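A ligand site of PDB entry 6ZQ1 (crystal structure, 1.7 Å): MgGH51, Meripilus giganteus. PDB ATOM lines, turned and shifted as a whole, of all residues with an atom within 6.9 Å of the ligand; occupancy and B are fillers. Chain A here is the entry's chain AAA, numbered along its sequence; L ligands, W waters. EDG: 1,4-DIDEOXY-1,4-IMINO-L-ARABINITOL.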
ATOM      1  N   MET A  21      -6.722 -31.965  -4.985  1.00  0.00           N
ATOM      2  CA  MET A  21      -7.968 -31.591  -4.253  1.00  0.00           C
ATOM      3  C   MET A  21      -8.823 -32.845  -4.136  1.00  0.00           C
ATOM      4  O   MET A  21      -9.224 -33.408  -5.167  1.00  0.00           O
ATOM      5  CB  MET A  21      -8.744 -30.515  -5.025  1.00  0.00           C
ATOM      6  CG  MET A  21     -10.038 -30.062  -4.337  1.00  0.00           C
ATOM      7  SD  MET A  21     -11.471 -31.047  -4.763  1.00  0.00           S
ATOM      8  CE  MET A  21     -12.656 -30.412  -3.601  1.00  0.00           C
ATOM      9  N   GLU A  23     -12.333 -34.681  -2.243  1.00  0.00           N
ATOM     10  CA  GLU A  23     -13.555 -34.946  -1.441  1.00  0.00           C
ATOM     11  C   GLU A  23     -14.090 -36.279  -1.928  1.00  0.00           C
ATOM     12  O   GLU A  23     -13.679 -36.733  -3.018  1.00  0.00           O
ATOM     13  CB  GLU A  23     -14.564 -33.815  -1.588  1.00  0.00           C
ATOM     14  CG  GLU A  23     -15.211 -33.811  -2.939  1.00  0.00           C
ATOM     15  CD  GLU A  23     -16.203 -32.689  -3.160  1.00  0.00           C
ATOM     16  OE1 GLU A  23     -17.142 -32.534  -2.329  1.00  0.00           O
ATOM     17  OE2 GLU A  23     -16.083 -32.051  -4.204  1.00  0.00           O
ATOM     18  N   ILE A  25     -16.511 -37.712  -3.825  1.00  0.00           N
ATOM     19  CA  ILE A  25     -17.410 -37.357  -4.965  1.00  0.00           C
ATOM     20  C   ILE A  25     -17.198 -38.427  -6.035  1.00  0.00           C
ATOM     21  O   ILE A  25     -16.045 -38.916  -6.140  1.00  0.00           O
ATOM     22  CB  ILE A  25     -17.128 -35.945  -5.504  1.00  0.00           C
ATOM     23  CG1 ILE A  25     -18.114 -35.545  -6.605  1.00  0.00           C
ATOM     24  CG2 ILE A  25     -15.690 -35.794  -5.936  1.00  0.00           C
ATOM     25  CD1 ILE A  25     -17.963 -34.097  -7.054  1.00  0.00           C
ATOM     26  N   ARG A 226      -5.555 -31.171  -0.467  1.00  0.00           N
ATOM     27  CA  ARG A 226      -6.696 -30.384   0.097  1.00  0.00           C
ATOM     28  C   ARG A 226      -7.857 -31.336   0.396  1.00  0.00           C
ATOM     29  O   ARG A 226      -8.204 -32.143  -0.477  1.00  0.00           O
ATOM     30  CB  ARG A 226      -7.122 -29.287  -0.877  1.00  0.00           C
ATOM     31  CG  ARG A 226      -8.240 -28.386  -0.357  1.00  0.00           C
ATOM     32  CD  ARG A 226      -8.923 -27.670  -1.521  1.00  0.00           C
ATOM     33  NE  ARG A 226     -10.045 -26.904  -1.027  1.00  0.00           N
ATOM     34  CZ  ARG A 226     -11.180 -26.642  -1.698  1.00  0.00           C
ATOM     35  NH1 ARG A 226     -11.351 -27.070  -2.949  1.00  0.00           N
ATOM     36  NH2 ARG A 226     -12.133 -25.966  -1.094  1.00  0.00           N
ATOM     37  N   GLY A 229     -13.021 -31.471   1.764  1.00  0.00           N
ATOM     38  CA  GLY A 229     -13.875 -30.898   0.691  1.00  0.00           C
ATOM     39  C   GLY A 229     -13.681 -29.403   0.681  1.00  0.00           C
ATOM     40  O   GLY A 229     -13.024 -28.875   1.580  1.00  0.00           O
ATOM     41  N   GLY A 230     -14.242 -28.702  -0.325  1.00  0.00           N
ATOM     42  CA  GLY A 230     -15.265 -29.276  -1.163  1.00  0.00           C
ATOM     43  C   GLY A 230     -16.636 -29.369  -0.494  1.00  0.00           C
ATOM     44  O   GLY A 230     -16.720 -29.294   0.791  1.00  0.00           O
ATOM     45  N   ASN A 231     -17.681 -29.554  -1.299  1.00  0.00           N
ATOM     46  CA  ASN A 231     -19.084 -29.626  -0.812  1.00  0.00           C
ATOM     47  C   ASN A 231     -19.213 -30.757   0.225  1.00  0.00           C
ATOM     48  O   ASN A 231     -20.035 -30.607   1.113  1.00  0.00           O
ATOM     49  CB  ASN A 231     -20.085 -29.862  -1.924  1.00  0.00           C
ATOM     50  CG  ASN A 231     -20.401 -28.567  -2.649  1.00  0.00           C
ATOM     51  OD1 ASN A 231     -19.744 -27.561  -2.414  1.00  0.00           O
ATOM     52  ND2 ASN A 231     -21.391 -28.637  -3.524  1.00  0.00           N
ATOM     53  N   ASN A 232     -18.393 -31.812   0.153  1.00  0.00           N
ATOM     54  CA  ASN A 232     -18.587 -32.986   1.048  1.00  0.00           C
ATOM     55  C   ASN A 232     -18.173 -32.611   2.482  1.00  0.00           C
ATOM     56  O   ASN A 232     -18.575 -33.383   3.438  1.00  0.00           O
ATOM     57  CB  ASN A 232     -17.916 -34.250   0.516  1.00  0.00           C
ATOM     58  CG  ASN A 232     -18.540 -35.524   1.012  1.00  0.00           C
ATOM     59  OD1 ASN A 232     -19.750 -35.692   0.867  1.00  0.00           O
ATOM     60  ND2 ASN A 232     -17.755 -36.350   1.750  1.00  0.00           N
ATOM     61  N   GLU A 234     -19.413 -29.786   3.940  1.00  0.00           N
ATOM     62  CA  GLU A 234     -20.435 -28.850   4.464  1.00  0.00           C
ATOM     63  C   GLU A 234     -21.659 -29.574   5.018  1.00  0.00           C
ATOM     64  O   GLU A 234     -22.256 -29.056   5.967  1.00  0.00           O
ATOM     65  CB  GLU A 234     -20.816 -27.894   3.340  1.00  0.00           C
ATOM     66  CG  GLU A 234     -19.704 -26.906   3.071  1.00  0.00           C
ATOM     67  CD  GLU A 234     -19.985 -26.057   1.831  1.00  0.00           C
ATOM     68  OE1 GLU A 234     -20.467 -24.949   2.007  1.00  0.00           O
ATOM     69  OE2 GLU A 234     -19.693 -26.501   0.725  1.00  0.00           O
ATOM     70  N   TRP A 261     -23.236 -35.880  -2.170  1.00  0.00           N
ATOM     71  CA  TRP A 261     -23.249 -36.290  -3.603  1.00  0.00           C
ATOM     72  C   TRP A 261     -24.138 -37.509  -3.833  1.00  0.00           C
ATOM     73  O   TRP A 261     -23.952 -38.206  -4.827  1.00  0.00           O
ATOM     74  CB  TRP A 261     -21.803 -36.461  -4.111  1.00  0.00           C
ATOM     75  CG  TRP A 261     -21.025 -35.184  -4.094  1.00  0.00           C
ATOM     76  CD1 TRP A 261     -19.997 -34.830  -3.248  1.00  0.00           C
ATOM     77  CD2 TRP A 261     -21.185 -34.081  -4.985  1.00  0.00           C
ATOM     78  NE1 TRP A 261     -19.538 -33.586  -3.553  1.00  0.00           N
ATOM     79  CE2 TRP A 261     -20.229 -33.104  -4.639  1.00  0.00           C
ATOM     80  CE3 TRP A 261     -22.015 -33.848  -6.077  1.00  0.00           C
ATOM     81  CZ2 TRP A 261     -20.106 -31.896  -5.298  1.00  0.00           C
ATOM     82  CZ3 TRP A 261     -21.898 -32.658  -6.744  1.00  0.00           C
ATOM     83  CH2 TRP A 261     -20.968 -31.677  -6.359  1.00  0.00           C
ATOM     84  N   ASN A 350     -15.987 -24.008   2.958  1.00  0.00           N
ATOM     85  CA  ASN A 350     -15.833 -24.250   1.510  1.00  0.00           C
ATOM     86  C   ASN A 350     -16.786 -23.314   0.773  1.00  0.00           C
ATOM     87  O   ASN A 350     -17.991 -23.308   1.143  1.00  0.00           O
ATOM     88  CB  ASN A 350     -16.237 -25.691   1.151  1.00  0.00           C
ATOM     89  CG  ASN A 350     -16.126 -25.962  -0.331  1.00  0.00           C
ATOM     90  OD1 ASN A 350     -15.025 -25.864  -0.867  1.00  0.00           O
ATOM     91  ND2 ASN A 350     -17.259 -26.256  -0.975  1.00  0.00           N
ATOM     92  N   GLU A 351     -16.286 -22.588  -0.202  1.00  0.00           N
ATOM     93  CA  GLU A 351     -17.109 -21.745  -1.110  1.00  0.00           C
ATOM     94  C   GLU A 351     -18.140 -20.962  -0.301  1.00  0.00           C
ATOM     95  O   GLU A 351     -19.354 -21.048  -0.606  1.00  0.00           O
ATOM     96  CB  GLU A 351     -17.790 -22.629  -2.164  1.00  0.00           C
ATOM     97  CG  GLU A 351     -16.802 -23.259  -3.139  1.00  0.00           C
ATOM     98  CD  GLU A 351     -17.363 -23.637  -4.510  1.00  0.00           C
ATOM     99  OE1 GLU A 351     -18.571 -23.992  -4.590  1.00  0.00           O
ATOM    100  OE2 GLU A 351     -16.560 -23.653  -5.486  1.00  0.00           O
ATOM    101  N   PHE A 353     -18.628 -17.926  -0.491  1.00  0.00           N
ATOM    102  CA  PHE A 353     -19.332 -16.968  -1.386  1.00  0.00           C
ATOM    103  C   PHE A 353     -20.799 -17.351  -1.553  1.00  0.00           C
ATOM    104  O   PHE A 353     -21.581 -16.490  -1.952  1.00  0.00           O
ATOM    105  CB  PHE A 353     -18.586 -16.798  -2.698  1.00  0.00           C
ATOM    106  CG  PHE A 353     -18.396 -18.044  -3.526  1.00  0.00           C
ATOM    107  CD1 PHE A 353     -19.438 -18.560  -4.300  1.00  0.00           C
ATOM    108  CD2 PHE A 353     -17.148 -18.636  -3.621  1.00  0.00           C
ATOM    109  CE1 PHE A 353     -19.243 -19.685  -5.097  1.00  0.00           C
ATOM    110  CE2 PHE A 353     -16.952 -19.760  -4.418  1.00  0.00           C
ATOM    111  CZ  PHE A 353     -17.998 -20.258  -5.180  1.00  0.00           C
ATOM    112  N   PHE A 354     -21.225 -18.580  -1.253  1.00  0.00           N
ATOM    113  CA  PHE A 354     -22.674 -18.938  -1.229  1.00  0.00           C
ATOM    114  C   PHE A 354     -23.368 -18.355   0.008  1.00  0.00           C
ATOM    115  O   PHE A 354     -24.615 -18.402   0.034  1.00  0.00           O
ATOM    116  CB  PHE A 354     -22.913 -20.449  -1.307  1.00  0.00           C
ATOM    117  CG  PHE A 354     -22.850 -21.019  -2.691  1.00  0.00           C
ATOM    118  CD1 PHE A 354     -23.940 -20.940  -3.549  1.00  0.00           C
ATOM    119  CD2 PHE A 354     -21.689 -21.625  -3.162  1.00  0.00           C
ATOM    120  CE1 PHE A 354     -23.882 -21.457  -4.840  1.00  0.00           C
ATOM    121  CE2 PHE A 354     -21.656 -22.180  -4.427  1.00  0.00           C
ATOM    122  CZ  PHE A 354     -22.728 -22.063  -5.282  1.00  0.00           C
ATOM    123  N   HIS A 400     -11.624 -20.627  -7.056  1.00  0.00           N
ATOM    124  CA  HIS A 400     -12.146 -21.762  -7.829  1.00  0.00           C
ATOM    125  C   HIS A 400     -12.572 -21.267  -9.220  1.00  0.00           C
ATOM    126  O   HIS A 400     -13.231 -20.214  -9.232  1.00  0.00           O
ATOM    127  CB  HIS A 400     -13.342 -22.391  -7.147  1.00  0.00           C
ATOM    128  CG  HIS A 400     -13.022 -23.013  -5.831  1.00  0.00           C
ATOM    129  ND1 HIS A 400     -13.978 -23.516  -4.986  1.00  0.00           N
ATOM    130  CD2 HIS A 400     -11.859 -23.116  -5.181  1.00  0.00           C
ATOM    131  CE1 HIS A 400     -13.400 -23.969  -3.884  1.00  0.00           C
ATOM    132  NE2 HIS A 400     -12.122 -23.705  -3.961  1.00  0.00           N
ATOM    133  N   TYR A 402     -14.263 -22.976 -13.069  1.00  0.00           N
ATOM    134  CA  TYR A 402     -14.693 -23.985 -14.045  1.00  0.00           C
ATOM    135  C   TYR A 402     -15.081 -23.207 -15.304  1.00  0.00           C
ATOM    136  O   TYR A 402     -15.949 -22.366 -15.173  1.00  0.00           O
ATOM    137  CB  TYR A 402     -15.821 -24.825 -13.476  1.00  0.00           C
ATOM    138  CG  TYR A 402     -15.386 -25.640 -12.271  1.00  0.00           C
ATOM    139  CD1 TYR A 402     -14.703 -26.829 -12.433  1.00  0.00           C
ATOM    140  CD2 TYR A 402     -15.646 -25.203 -10.986  1.00  0.00           C
ATOM    141  CE1 TYR A 402     -14.305 -27.597 -11.334  1.00  0.00           C
ATOM    142  CE2 TYR A 402     -15.253 -25.962  -9.879  1.00  0.00           C
ATOM    143  CZ  TYR A 402     -14.595 -27.167 -10.064  1.00  0.00           C
ATOM    144  OH  TYR A 402     -14.220 -27.917  -8.993  1.00  0.00           O
ATOM    145  N   GLU A 429      -9.532 -25.290  -6.842  1.00  0.00           N
ATOM    146  CA  GLU A 429     -10.292 -26.089  -7.801  1.00  0.00           C
ATOM    147  C   GLU A 429     -10.239 -25.349  -9.138  1.00  0.00           C
ATOM    148  O   GLU A 429     -10.590 -24.172  -9.140  1.00  0.00           O
ATOM    149  CB  GLU A 429     -11.783 -26.206  -7.462  1.00  0.00           C
ATOM    150  CG  GLU A 429     -12.056 -26.844  -6.093  1.00  0.00           C
ATOM    151  CD  GLU A 429     -13.525 -26.863  -5.708  1.00  0.00           C
ATOM    152  OE1 GLU A 429     -14.429 -26.736  -6.631  1.00  0.00           O
ATOM    153  OE2 GLU A 429     -13.800 -27.007  -4.513  1.00  0.00           O
ATOM    154  N   ALA A 480      -9.750 -29.972 -10.109  1.00  0.00           N
ATOM    155  CA  ALA A 480     -10.876 -30.693  -9.448  1.00  0.00           C
ATOM    156  C   ALA A 480     -11.970 -31.035 -10.432  1.00  0.00           C
ATOM    157  O   ALA A 480     -12.204 -30.282 -11.378  1.00  0.00           O
ATOM    158  CB  ALA A 480     -11.401 -29.885  -8.280  1.00  0.00           C
ATOM    159  N   PRO A 481     -12.722 -32.143 -10.203  1.00  0.00           N
ATOM    160  CA  PRO A 481     -12.413 -33.153  -9.190  1.00  0.00           C
ATOM    161  C   PRO A 481     -11.256 -34.090  -9.600  1.00  0.00           C
ATOM    162  O   PRO A 481     -10.951 -34.253 -10.761  1.00  0.00           O
ATOM    163  CB  PRO A 481     -13.736 -33.927  -9.052  1.00  0.00           C
ATOM    164  CG  PRO A 481     -14.782 -33.021  -9.679  1.00  0.00           C
ATOM    165  CD  PRO A 481     -14.025 -32.412 -10.833  1.00  0.00           C
ATOM    166  N   LEU A 482     -10.673 -34.748  -8.605  1.00  0.00           N
ATOM    167  CA  LEU A 482      -9.513 -35.635  -8.816  1.00  0.00           C
ATOM    168  C   LEU A 482      -9.930 -36.978  -9.446  1.00  0.00           C
ATOM    169  O   LEU A 482      -9.239 -37.440 -10.331  1.00  0.00           O
ATOM    170  CB  LEU A 482      -8.861 -35.810  -7.441  1.00  0.00           C
ATOM    171  CG  LEU A 482      -7.607 -36.663  -7.379  1.00  0.00           C
ATOM    172  CD1 LEU A 482      -6.485 -36.089  -8.220  1.00  0.00           C
ATOM    173  CD2 LEU A 482      -7.154 -36.840  -5.930  1.00  0.00           C
ATOM    174  N   TRP A 491     -20.195 -35.742 -11.419  1.00  0.00           N
ATOM    175  CA  TRP A 491     -19.465 -34.592 -11.994  1.00  0.00           C
ATOM    176  C   TRP A 491     -18.412 -35.066 -12.982  1.00  0.00           C
ATOM    177  O   TRP A 491     -17.634 -35.964 -12.627  1.00  0.00           O
ATOM    178  CB  TRP A 491     -18.809 -33.793 -10.880  1.00  0.00           C
ATOM    179  CG  TRP A 491     -18.143 -32.540 -11.357  1.00  0.00           C
ATOM    180  CD1 TRP A 491     -17.023 -32.414 -12.132  1.00  0.00           C
ATOM    181  CD2 TRP A 491     -18.574 -31.218 -11.033  1.00  0.00           C
ATOM    182  NE1 TRP A 491     -16.744 -31.083 -12.322  1.00  0.00           N
ATOM    183  CE2 TRP A 491     -17.685 -30.322 -11.687  1.00  0.00           C
ATOM    184  CE3 TRP A 491     -19.608 -30.687 -10.267  1.00  0.00           C
ATOM    185  CZ2 TRP A 491     -17.782 -28.939 -11.536  1.00  0.00           C
ATOM    186  CZ3 TRP A 491     -19.720 -29.322 -10.143  1.00  0.00           C
ATOM    187  CH2 TRP A 491     -18.808 -28.459 -10.765  1.00  0.00           C
HETATM  188  O2' EDG L   1     -16.470 -26.917  -3.812  1.00  0.00           O
HETATM  189  C2' EDG L   1     -17.337 -27.553  -4.729  1.00  0.00           C
HETATM  190  C1' EDG L   1     -17.433 -26.767  -6.037  1.00  0.00           C
HETATM  191  N4' EDG L   1     -17.095 -27.765  -7.047  1.00  0.00           N
HETATM  192  C3' EDG L   1     -16.891 -28.976  -5.093  1.00  0.00           C
HETATM  193  O3' EDG L   1     -17.521 -29.922  -4.223  1.00  0.00           O
HETATM  194  C4' EDG L   1     -17.347 -29.136  -6.547  1.00  0.00           C
HETATM  195  C5' EDG L   1     -16.665 -30.259  -7.311  1.00  0.00           C
HETATM  196  O5' EDG L   1     -15.258 -30.097  -7.378  1.00  0.00           O
HETATM  197  O   HOH W   1     -14.092 -32.376  -6.046  1.00  0.00           O
HETATM  198  O   HOH W   2     -18.660 -25.369  -8.939  1.00  0.00           O
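N of Asn 231 lies within hydrogen-bond range of O3' of the ligand, 3.0 Å away. OH of Tyr 402 is in hydrogen-bond range of O5' of the ligand (2.9 Å). OE1 of Glu 429 is in salt-bridge range of N4' of the ligand (2.9 Å). The side-chain amide nitrogen (ND2) of Asn 350 is in hydrogen-bond range of an oxygen (O2') of the ligand (3.0 Å). OE2 of Glu 23 sits at hydrogen-bond distance from O3' of the ligand, at 2.6 Å.
NH1 of Arg 226 lies within salt-bridge range of OE2 of Glu 429 (2.9 Å). The side-chain amide oxygen of Asn 231 is in hydrogen-bond range of the side-chain amide nitrogen of Asn 350, 3.2 Å away. The side-chain carboxylate of Glu 23 sits at hydrogen-bond distance from the backbone NH of Asn 232, at 2.9 Å. N of Gly 230 sits at hydrogen-bond distance from OD1 of Asn 350 (3.0 Å). The side-chain carboxylate (OE1) of Glu 23 sits at hydrogen-bond distance from the indole nitrogen (NE1) of Trp 261 (2.9 Å). The side-chain carboxylate (OE2) of Glu 351 is in hydrogen-bond range of a ring nitrogen (ND1) of His 400, at 2.6 Å. The side-chain amide oxygen (OD1) of Asn 350 sits at hydrogen-bond distance from the guanidinium group (NH2) of Arg 226, at 2.9 Å. The side-chain amide oxygen (OD1) of Asn 231 lies close to the side-chain carboxylate (OE2) of Glu 234 (3.3 Å).
Residues that only touch the ligand: Glu 351 (3.3 Å), Trp 261 (3.4 Å), Gly 230 (3.7 Å), Pro 481 (3.8 Å) and Ala 480 (3.97 Å). Hydrophobic or aromatic side chains that line the ligand: Trp 261, Tyr 402, Ala 480 and Pro 481. Ten residues have an atom within 4 Å of the ligand: Glu 23, Gly 230, Asn 231, Trp 261, Asn 350, Glu 351, Tyr 402, Glu 429, Ala 480 and Pro 481. The nearest printed residue that does not touch the ligand is Ile 25 (4.1 Å).
Water W1 lies within hydrogen-bond range of OE2 of Glu 23 (2.7 Å), O5' of the ligand (2.9 Å) and SD of Met 21 (3.2 Å).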
